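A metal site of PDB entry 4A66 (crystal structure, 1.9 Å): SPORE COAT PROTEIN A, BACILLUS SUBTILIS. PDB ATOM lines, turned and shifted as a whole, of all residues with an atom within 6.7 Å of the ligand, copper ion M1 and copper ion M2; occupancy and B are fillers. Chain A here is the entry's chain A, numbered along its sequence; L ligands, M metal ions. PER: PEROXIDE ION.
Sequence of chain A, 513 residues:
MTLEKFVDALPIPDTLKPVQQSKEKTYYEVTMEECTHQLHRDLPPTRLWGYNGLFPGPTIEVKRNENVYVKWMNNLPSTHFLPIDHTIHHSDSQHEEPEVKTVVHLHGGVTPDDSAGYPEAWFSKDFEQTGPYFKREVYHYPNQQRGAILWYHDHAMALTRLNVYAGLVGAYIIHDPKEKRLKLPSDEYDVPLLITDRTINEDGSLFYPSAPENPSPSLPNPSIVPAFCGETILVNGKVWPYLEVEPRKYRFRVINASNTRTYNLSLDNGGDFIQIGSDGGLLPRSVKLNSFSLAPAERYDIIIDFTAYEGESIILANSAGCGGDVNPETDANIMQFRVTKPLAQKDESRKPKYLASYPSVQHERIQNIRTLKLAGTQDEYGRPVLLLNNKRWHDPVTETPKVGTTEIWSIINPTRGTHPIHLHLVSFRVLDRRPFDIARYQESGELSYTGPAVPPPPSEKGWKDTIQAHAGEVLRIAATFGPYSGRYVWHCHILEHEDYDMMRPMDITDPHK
N of His 424 lies within hydrogen-bond range of O of Val 489 (3.0 Å). NE2 of His 107 lies close to ND1 of His 422, 3.4 Å away. N of His 107 lies within hydrogen-bond range of O of Trp 151, 2.8 Å away. A ring nitrogen (NE2) of His 107 is in hydrogen-bond range of the side-chain hydroxyl (OG1) of Thr 466, 3.2 Å away. N of His 105 lies within hydrogen-bond range of O of His 153 (2.8 Å). The backbone NH (N) of His 422 sits at hydrogen-bond distance from the backbone carbonyl oxygen (O) of His 491 (2.7 Å). ND1 of His 491 sits at hydrogen-bond distance from OE1 of Glu 498 (3.0 Å). A ring nitrogen (ND1) of His 422 lies within hydrogen-bond range of the side-chain hydroxyl (OG1) of Thr 466 (3.1 Å).
NE2 of His 105 sits close to O2 of the ligand, at 3.0 Å. An oxygen (O2) of the ligand lies close to a ring nitrogen (NE2) of His 422 (3.4 Å). Hydrophobic or aromatic side chains within 4 Å of the ligand: His 105, His 107, His 153, His 155, His 422, His 491 and His 493.
Merely in contact with copper ion M1: His 105 (3.8 Å) and Trp 151 (3.8 Å). Within 4 Å of copper ion M1: His 105, His 107, Trp 151, His 153 and His 493. The nearest printed residue that does not touch copper ion M1 is Ala 297 (4.4 Å).
Merely in contact with copper ion M2: His 105 (3.8 Å) and His 422 (3.8 Å). Along chain A the residues within 4 Å of copper ion M2 span positions 105 to 491. The nearest printed residue that does not touch copper ion M2 is Glu 498 (4.6 Å).
A ring nitrogen (ND1) of His 107 binds copper ion M1 (2.0 Å). NE2 of His 153 is bound to copper ion M1. Copper ion M1 is bound by a ring nitrogen (NE2) of His 493 (2.1 Å). An oxygen (O2) of the ligand binds copper ion M1 (2.3 Å). Copper ion M1 has four donor atoms within binding distance.
Copper ion M2 is bound by a ring nitrogen (NE2) of His 424 (2.0 Å), a ring nitrogen (NE2) of His 155 (2.0 Å), a ring nitrogen (NE2) of His 491 (2.0 Å) and an oxygen (O1) of the ligand (2.1 Å).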
ATOM      1  N   HIS A 105      -6.456 -15.316   3.901  1.00  0.00           N
ATOM      2  CA  HIS A 105      -7.199 -16.392   3.264  1.00  0.00           C
ATOM      3  C   HIS A 105      -8.398 -15.791   2.553  1.00  0.00           C
ATOM      4  O   HIS A 105      -9.209 -15.084   3.175  1.00  0.00           O
ATOM      5  CB  HIS A 105      -7.686 -17.378   4.350  1.00  0.00           C
ATOM      6  CG  HIS A 105      -8.638 -18.405   3.834  1.00  0.00           C
ATOM      7  ND1 HIS A 105      -8.310 -19.297   2.839  1.00  0.00           N
ATOM      8  CD2 HIS A 105      -9.908 -18.703   4.198  1.00  0.00           C
ATOM      9  CE1 HIS A 105      -9.334 -20.106   2.612  1.00  0.00           C
ATOM     10  NE2 HIS A 105     -10.313 -19.746   3.426  1.00  0.00           N
ATOM     11  N   LEU A 106      -8.473 -16.027   1.235  1.00  0.00           N
ATOM     12  CA  LEU A 106      -9.670 -15.685   0.455  1.00  0.00           C
ATOM     13  C   LEU A 106     -10.655 -16.826   0.640  1.00  0.00           C
ATOM     14  O   LEU A 106     -10.549 -17.881  -0.003  1.00  0.00           O
ATOM     15  CB  LEU A 106      -9.349 -15.484  -1.044  1.00  0.00           C
ATOM     16  CG  LEU A 106     -10.588 -15.078  -1.904  1.00  0.00           C
ATOM     17  CD1 LEU A 106     -11.277 -13.763  -1.334  1.00  0.00           C
ATOM     18  CD2 LEU A 106     -10.155 -14.863  -3.345  1.00  0.00           C
ATOM     19  N   HIS A 107     -11.592 -16.629   1.565  1.00  0.00           N
ATOM     20  CA  HIS A 107     -12.574 -17.645   1.932  1.00  0.00           C
ATOM     21  C   HIS A 107     -13.570 -17.875   0.784  1.00  0.00           C
ATOM     22  O   HIS A 107     -14.259 -16.949   0.373  1.00  0.00           O
ATOM     23  CB  HIS A 107     -13.339 -17.192   3.169  1.00  0.00           C
ATOM     24  CG  HIS A 107     -14.313 -18.198   3.666  1.00  0.00           C
ATOM     25  ND1 HIS A 107     -14.194 -18.797   4.902  1.00  0.00           N
ATOM     26  CD2 HIS A 107     -15.397 -18.773   3.071  1.00  0.00           C
ATOM     27  CE1 HIS A 107     -15.191 -19.654   5.071  1.00  0.00           C
ATOM     28  NE2 HIS A 107     -15.918 -19.680   3.968  1.00  0.00           N
ATOM     29  N   GLY A 108     -13.652 -19.113   0.314  1.00  0.00           N
ATOM     30  CA  GLY A 108     -14.422 -19.443  -0.885  1.00  0.00           C
ATOM     31  C   GLY A 108     -13.618 -19.294  -2.183  1.00  0.00           C
ATOM     32  O   GLY A 108     -14.114 -19.665  -3.235  1.00  0.00           O
ATOM     33  N   GLY A 117      -3.763 -18.991   1.400  1.00  0.00           N
ATOM     34  CA  GLY A 117      -3.633 -18.502   2.785  1.00  0.00           C
ATOM     35  C   GLY A 117      -3.603 -19.651   3.793  1.00  0.00           C
ATOM     36  O   GLY A 117      -4.316 -19.662   4.794  1.00  0.00           O
ATOM     37  N   PRO A 119      -2.568 -21.913   6.826  1.00  0.00           N
ATOM     38  CA  PRO A 119      -2.266 -21.409   8.162  1.00  0.00           C
ATOM     39  C   PRO A 119      -0.757 -21.413   8.469  1.00  0.00           C
ATOM     40  O   PRO A 119      -0.313 -20.611   9.268  1.00  0.00           O
ATOM     41  CB  PRO A 119      -3.000 -22.355   9.120  1.00  0.00           C
ATOM     42  CG  PRO A 119      -3.938 -23.186   8.248  1.00  0.00           C
ATOM     43  CD  PRO A 119      -3.502 -23.061   6.837  1.00  0.00           C
ATOM     44  N   TRP A 151     -15.156 -13.605   1.168  1.00  0.00           N
ATOM     45  CA  TRP A 151     -14.624 -12.631   2.116  1.00  0.00           C
ATOM     46  C   TRP A 151     -13.191 -13.054   2.413  1.00  0.00           C
ATOM     47  O   TRP A 151     -12.798 -14.175   2.099  1.00  0.00           O
ATOM     48  CB  TRP A 151     -15.508 -12.508   3.376  1.00  0.00           C
ATOM     49  CG  TRP A 151     -15.600 -13.722   4.321  1.00  0.00           C
ATOM     50  CD1 TRP A 151     -16.147 -14.964   4.033  1.00  0.00           C
ATOM     51  CD2 TRP A 151     -15.228 -13.751   5.708  1.00  0.00           C
ATOM     52  NE1 TRP A 151     -16.103 -15.761   5.173  1.00  0.00           N
ATOM     53  CE2 TRP A 151     -15.545 -15.054   6.204  1.00  0.00           C
ATOM     54  CE3 TRP A 151     -14.647 -12.814   6.585  1.00  0.00           C
ATOM     55  CZ2 TRP A 151     -15.300 -15.434   7.528  1.00  0.00           C
ATOM     56  CZ3 TRP A 151     -14.414 -13.177   7.901  1.00  0.00           C
ATOM     57  CH2 TRP A 151     -14.721 -14.486   8.368  1.00  0.00           C
ATOM     58  N   HIS A 153      -9.834 -12.912   5.241  1.00  0.00           N
ATOM     59  CA  HIS A 153      -9.533 -12.773   6.646  1.00  0.00           C
ATOM     60  C   HIS A 153      -8.205 -13.467   6.969  1.00  0.00           C
ATOM     61  O   HIS A 153      -7.715 -14.322   6.186  1.00  0.00           O
ATOM     62  CB  HIS A 153     -10.676 -13.333   7.515  1.00  0.00           C
ATOM     63  CG  HIS A 153     -10.944 -14.797   7.326  1.00  0.00           C
ATOM     64  ND1 HIS A 153     -10.224 -15.778   7.985  1.00  0.00           N
ATOM     65  CD2 HIS A 153     -11.874 -15.440   6.582  1.00  0.00           C
ATOM     66  CE1 HIS A 153     -10.696 -16.968   7.638  1.00  0.00           C
ATOM     67  NE2 HIS A 153     -11.703 -16.786   6.795  1.00  0.00           N
ATOM     68  N   ASP A 154      -7.608 -13.066   8.094  1.00  0.00           N
ATOM     69  CA  ASP A 154      -6.366 -13.704   8.537  1.00  0.00           C
ATOM     70  C   ASP A 154      -6.625 -15.184   8.850  1.00  0.00           C
ATOM     71  O   ASP A 154      -7.715 -15.557   9.291  1.00  0.00           O
ATOM     72  CB  ASP A 154      -5.830 -13.026   9.803  1.00  0.00           C
ATOM     73  CG  ASP A 154      -4.414 -13.485  10.100  1.00  0.00           C
ATOM     74  OD1 ASP A 154      -3.502 -13.054   9.369  1.00  0.00           O
ATOM     75  OD2 ASP A 154      -4.267 -14.339  10.974  1.00  0.00           O
ATOM     76  N   HIS A 155      -5.598 -15.999   8.647  1.00  0.00           N
ATOM     77  CA  HIS A 155      -5.716 -17.427   8.859  1.00  0.00           C
ATOM     78  C   HIS A 155      -4.441 -17.999   9.539  1.00  0.00           C
ATOM     79  O   HIS A 155      -4.176 -19.197   9.432  1.00  0.00           O
ATOM     80  CB  HIS A 155      -5.944 -18.134   7.514  1.00  0.00           C
ATOM     81  CG  HIS A 155      -6.793 -19.366   7.592  1.00  0.00           C
ATOM     82  ND1 HIS A 155      -6.541 -20.404   8.463  1.00  0.00           N
ATOM     83  CD2 HIS A 155      -7.922 -19.722   6.906  1.00  0.00           C
ATOM     84  CE1 HIS A 155      -7.461 -21.350   8.310  1.00  0.00           C
ATOM     85  NE2 HIS A 155      -8.302 -20.973   7.359  1.00  0.00           N
ATOM     86  N   THR A 160      -5.542 -17.223  14.562  1.00  0.00           N
ATOM     87  CA  THR A 160      -6.715 -16.804  13.755  1.00  0.00           C
ATOM     88  C   THR A 160      -7.779 -16.069  14.574  1.00  0.00           C
ATOM     89  O   THR A 160      -8.246 -14.995  14.169  1.00  0.00           O
ATOM     90  CB  THR A 160      -7.242 -18.011  12.950  1.00  0.00           C
ATOM     91  OG1 THR A 160      -6.185 -18.410  12.052  1.00  0.00           O
ATOM     92  CG2 THR A 160      -8.452 -17.641  12.095  1.00  0.00           C
ATOM     93  N   ALA A 297     -18.852 -17.500   9.086  1.00  0.00           N
ATOM     94  CA  ALA A 297     -18.370 -17.664   7.693  1.00  0.00           C
ATOM     95  C   ALA A 297     -19.426 -17.963   6.634  1.00  0.00           C
ATOM     96  O   ALA A 297     -19.127 -17.889   5.453  1.00  0.00           O
ATOM     97  CB  ALA A 297     -17.191 -18.650   7.610  1.00  0.00           C
ATOM     98  N   HIS A 422     -16.146 -26.100   7.453  1.00  0.00           N
ATOM     99  CA  HIS A 422     -15.745 -25.431   6.248  1.00  0.00           C
ATOM    100  C   HIS A 422     -14.654 -26.210   5.511  1.00  0.00           C
ATOM    101  O   HIS A 422     -13.692 -26.687   6.137  1.00  0.00           O
ATOM    102  CB  HIS A 422     -15.278 -24.005   6.591  1.00  0.00           C
ATOM    103  CG  HIS A 422     -14.657 -23.275   5.440  1.00  0.00           C
ATOM    104  ND1 HIS A 422     -15.314 -23.059   4.251  1.00  0.00           N
ATOM    105  CD2 HIS A 422     -13.444 -22.699   5.316  1.00  0.00           C
ATOM    106  CE1 HIS A 422     -14.520 -22.384   3.430  1.00  0.00           C
ATOM    107  NE2 HIS A 422     -13.379 -22.157   4.059  1.00  0.00           N
ATOM    108  N   LEU A 423     -14.805 -26.354   4.193  1.00  0.00           N
ATOM    109  CA  LEU A 423     -13.753 -26.950   3.364  1.00  0.00           C
ATOM    110  C   LEU A 423     -13.157 -25.845   2.510  1.00  0.00           C
ATOM    111  O   LEU A 423     -13.883 -25.106   1.874  1.00  0.00           O
ATOM    112  CB  LEU A 423     -14.323 -28.049   2.448  1.00  0.00           C
ATOM    113  CG  LEU A 423     -14.488 -29.480   3.032  1.00  0.00           C
ATOM    114  CD1 LEU A 423     -15.490 -29.469   4.196  1.00  0.00           C
ATOM    115  CD2 LEU A 423     -14.917 -30.485   1.899  1.00  0.00           C
ATOM    116  N   HIS A 424     -11.832 -25.723   2.480  1.00  0.00           N
ATOM    117  CA  HIS A 424     -11.205 -24.768   1.557  1.00  0.00           C
ATOM    118  C   HIS A 424     -11.363 -25.255   0.130  1.00  0.00           C
ATOM    119  O   HIS A 424     -11.701 -26.419  -0.089  1.00  0.00           O
ATOM    120  CB  HIS A 424      -9.701 -24.636   1.858  1.00  0.00           C
ATOM    121  CG  HIS A 424      -9.402 -23.843   3.083  1.00  0.00           C
ATOM    122  ND1 HIS A 424      -8.173 -23.246   3.294  1.00  0.00           N
ATOM    123  CD2 HIS A 424     -10.168 -23.515   4.161  1.00  0.00           C
ATOM    124  CE1 HIS A 424      -8.184 -22.627   4.464  1.00  0.00           C
ATOM    125  NE2 HIS A 424      -9.380 -22.767   5.017  1.00  0.00           N
ATOM    126  N   THR A 466     -19.485 -23.586   3.914  1.00  0.00           N
ATOM    127  CA  THR A 466     -19.474 -23.616   5.358  1.00  0.00           C
ATOM    128  C   THR A 466     -20.862 -24.088   5.799  1.00  0.00           C
ATOM    129  O   THR A 466     -21.853 -23.516   5.393  1.00  0.00           O
ATOM    130  CB  THR A 466     -19.159 -22.222   5.954  1.00  0.00           C
ATOM    131  OG1 THR A 466     -17.927 -21.720   5.387  1.00  0.00           O
ATOM    132  CG2 THR A 466     -19.035 -22.294   7.478  1.00  0.00           C
ATOM    133  N   VAL A 489      -7.136 -27.273   3.412  1.00  0.00           N
ATOM    134  CA  VAL A 489      -7.524 -27.399   4.820  1.00  0.00           C
ATOM    135  C   VAL A 489      -9.017 -27.672   4.906  1.00  0.00           C
ATOM    136  O   VAL A 489      -9.751 -27.290   4.012  1.00  0.00           O
ATOM    137  CB  VAL A 489      -7.260 -26.054   5.613  1.00  0.00           C
ATOM    138  CG1 VAL A 489      -7.612 -26.228   7.128  1.00  0.00           C
ATOM    139  CG2 VAL A 489      -5.787 -25.582   5.492  1.00  0.00           C
ATOM    140  N   TRP A 490      -9.480 -28.348   5.972  1.00  0.00           N
ATOM    141  CA  TRP A 490     -10.891 -28.299   6.327  1.00  0.00           C
ATOM    142  C   TRP A 490     -10.954 -28.147   7.838  1.00  0.00           C
ATOM    143  O   TRP A 490     -10.060 -28.645   8.541  1.00  0.00           O
ATOM    144  CB  TRP A 490     -11.650 -29.543   5.814  1.00  0.00           C
ATOM    145  CG  TRP A 490     -11.377 -30.827   6.589  1.00  0.00           C
ATOM    146  CD1 TRP A 490     -10.247 -31.622   6.527  1.00  0.00           C
ATOM    147  CD2 TRP A 490     -12.264 -31.455   7.507  1.00  0.00           C
ATOM    148  NE1 TRP A 490     -10.378 -32.707   7.401  1.00  0.00           N
ATOM    149  CE2 TRP A 490     -11.609 -32.630   7.997  1.00  0.00           C
ATOM    150  CE3 TRP A 490     -13.546 -31.144   7.986  1.00  0.00           C
ATOM    151  CZ2 TRP A 490     -12.220 -33.481   8.916  1.00  0.00           C
ATOM    152  CZ3 TRP A 490     -14.149 -31.999   8.908  1.00  0.00           C
ATOM    153  CH2 TRP A 490     -13.481 -33.159   9.357  1.00  0.00           C
ATOM    154  N   HIS A 491     -11.949 -27.443   8.332  1.00  0.00           N
ATOM    155  CA  HIS A 491     -11.950 -27.034   9.740  1.00  0.00           C
ATOM    156  C   HIS A 491     -13.319 -26.526  10.194  1.00  0.00           C
ATOM    157  O   HIS A 491     -14.186 -26.201   9.351  1.00  0.00           O
ATOM    158  CB  HIS A 491     -10.885 -25.944  10.014  1.00  0.00           C
ATOM    159  CG  HIS A 491     -11.096 -24.634   9.288  1.00  0.00           C
ATOM    160  ND1 HIS A 491     -11.661 -23.523   9.898  1.00  0.00           N
ATOM    161  CD2 HIS A 491     -10.752 -24.250   8.042  1.00  0.00           C
ATOM    162  CE1 HIS A 491     -11.681 -22.521   9.030  1.00  0.00           C
ATOM    163  NE2 HIS A 491     -11.089 -22.921   7.914  1.00  0.00           N
ATOM    164  N   CYS A 492     -13.513 -26.492  11.498  1.00  0.00           N
ATOM    165  CA  CYS A 492     -14.626 -25.750  12.083  1.00  0.00           C
ATOM    166  C   CYS A 492     -14.302 -24.264  12.008  1.00  0.00           C
ATOM    167  O   CYS A 492     -13.174 -23.883  12.268  1.00  0.00           O
ATOM    168  CB  CYS A 492     -14.835 -26.141  13.529  1.00  0.00           C
ATOM    169  SG  CYS A 492     -16.104 -25.174  14.307  1.00  0.00           S
ATOM    170  N   HIS A 493     -15.283 -23.438  11.664  1.00  0.00           N
ATOM    171  CA  HIS A 493     -15.044 -22.002  11.482  1.00  0.00           C
ATOM    172  C   HIS A 493     -15.451 -21.188  12.734  1.00  0.00           C
ATOM    173  O   HIS A 493     -15.522 -19.953  12.686  1.00  0.00           O
ATOM    174  CB  HIS A 493     -15.728 -21.464  10.189  1.00  0.00           C
ATOM    175  CG  HIS A 493     -14.927 -20.388   9.488  1.00  0.00           C
ATOM    176  ND1 HIS A 493     -14.697 -19.143  10.062  1.00  0.00           N
ATOM    177  CD2 HIS A 493     -14.313 -20.357   8.276  1.00  0.00           C
ATOM    178  CE1 HIS A 493     -13.963 -18.405   9.230  1.00  0.00           C
ATOM    179  NE2 HIS A 493     -13.719 -19.114   8.138  1.00  0.00           N
ATOM    180  N   LEU A 495     -13.662 -19.841  15.466  1.00  0.00           N
ATOM    181  CA  LEU A 495     -12.227 -19.582  15.470  1.00  0.00           C
ATOM    182  C   LEU A 495     -11.568 -20.087  16.749  1.00  0.00           C
ATOM    183  O   LEU A 495     -10.439 -20.558  16.710  1.00  0.00           O
ATOM    184  CB  LEU A 495     -11.950 -18.099  15.228  1.00  0.00           C
ATOM    185  CG  LEU A 495     -12.556 -17.554  13.928  1.00  0.00           C
ATOM    186  CD1 LEU A 495     -12.001 -16.127  13.698  1.00  0.00           C
ATOM    187  CD2 LEU A 495     -12.205 -18.451  12.716  1.00  0.00           C
ATOM    188  N   GLU A 498     -11.229 -23.751  15.872  1.00  0.00           N
ATOM    189  CA  GLU A 498     -10.189 -23.811  14.839  1.00  0.00           C
ATOM    190  C   GLU A 498      -8.752 -23.763  15.391  1.00  0.00           C
ATOM    191  O   GLU A 498      -7.865 -24.548  14.971  1.00  0.00           O
ATOM    192  CB  GLU A 498     -10.419 -22.664  13.847  1.00  0.00           C
ATOM    193  CG  GLU A 498      -9.390 -22.564  12.768  1.00  0.00           C
ATOM    194  CD  GLU A 498      -9.759 -21.540  11.718  1.00  0.00           C
ATOM    195  OE1 GLU A 498     -10.958 -21.182  11.603  1.00  0.00           O
ATOM    196  OE2 GLU A 498      -8.845 -21.109  11.009  1.00  0.00           O
ATOM    197  N   MET A 503      -8.988 -28.391  13.085  1.00  0.00           N
ATOM    198  CA  MET A 503      -8.541 -28.036  11.762  1.00  0.00           C
ATOM    199  C   MET A 503      -7.590 -29.097  11.279  1.00  0.00           C
ATOM    200  O   MET A 503      -6.693 -29.484  12.015  1.00  0.00           O
ATOM    201  CB  MET A 503      -7.800 -26.682  11.816  1.00  0.00           C
ATOM    202  CG  MET A 503      -7.307 -26.172  10.448  1.00  0.00           C
ATOM    203  SD  MET A 503      -6.686 -24.461  10.456  1.00  0.00           S
ATOM    204  CE  MET A 503      -5.082 -24.611  11.277  1.00  0.00           C
HETATM  205  O1  PER L   1     -11.003 -20.125   7.470  1.00  0.00           O
HETATM  206  O2  PER L   1     -11.587 -20.136   6.167  1.00  0.00           O
HETATM  207 CU    CU M   1     -12.988 -18.294   6.405  1.00  0.00          CU
HETATM  208 CU    CU M   2     -10.011 -21.771   6.618  1.00  0.00          CU
HETATM  209 CU    CU M   3     -11.868 -20.966   3.630  1.00  0.00          CU
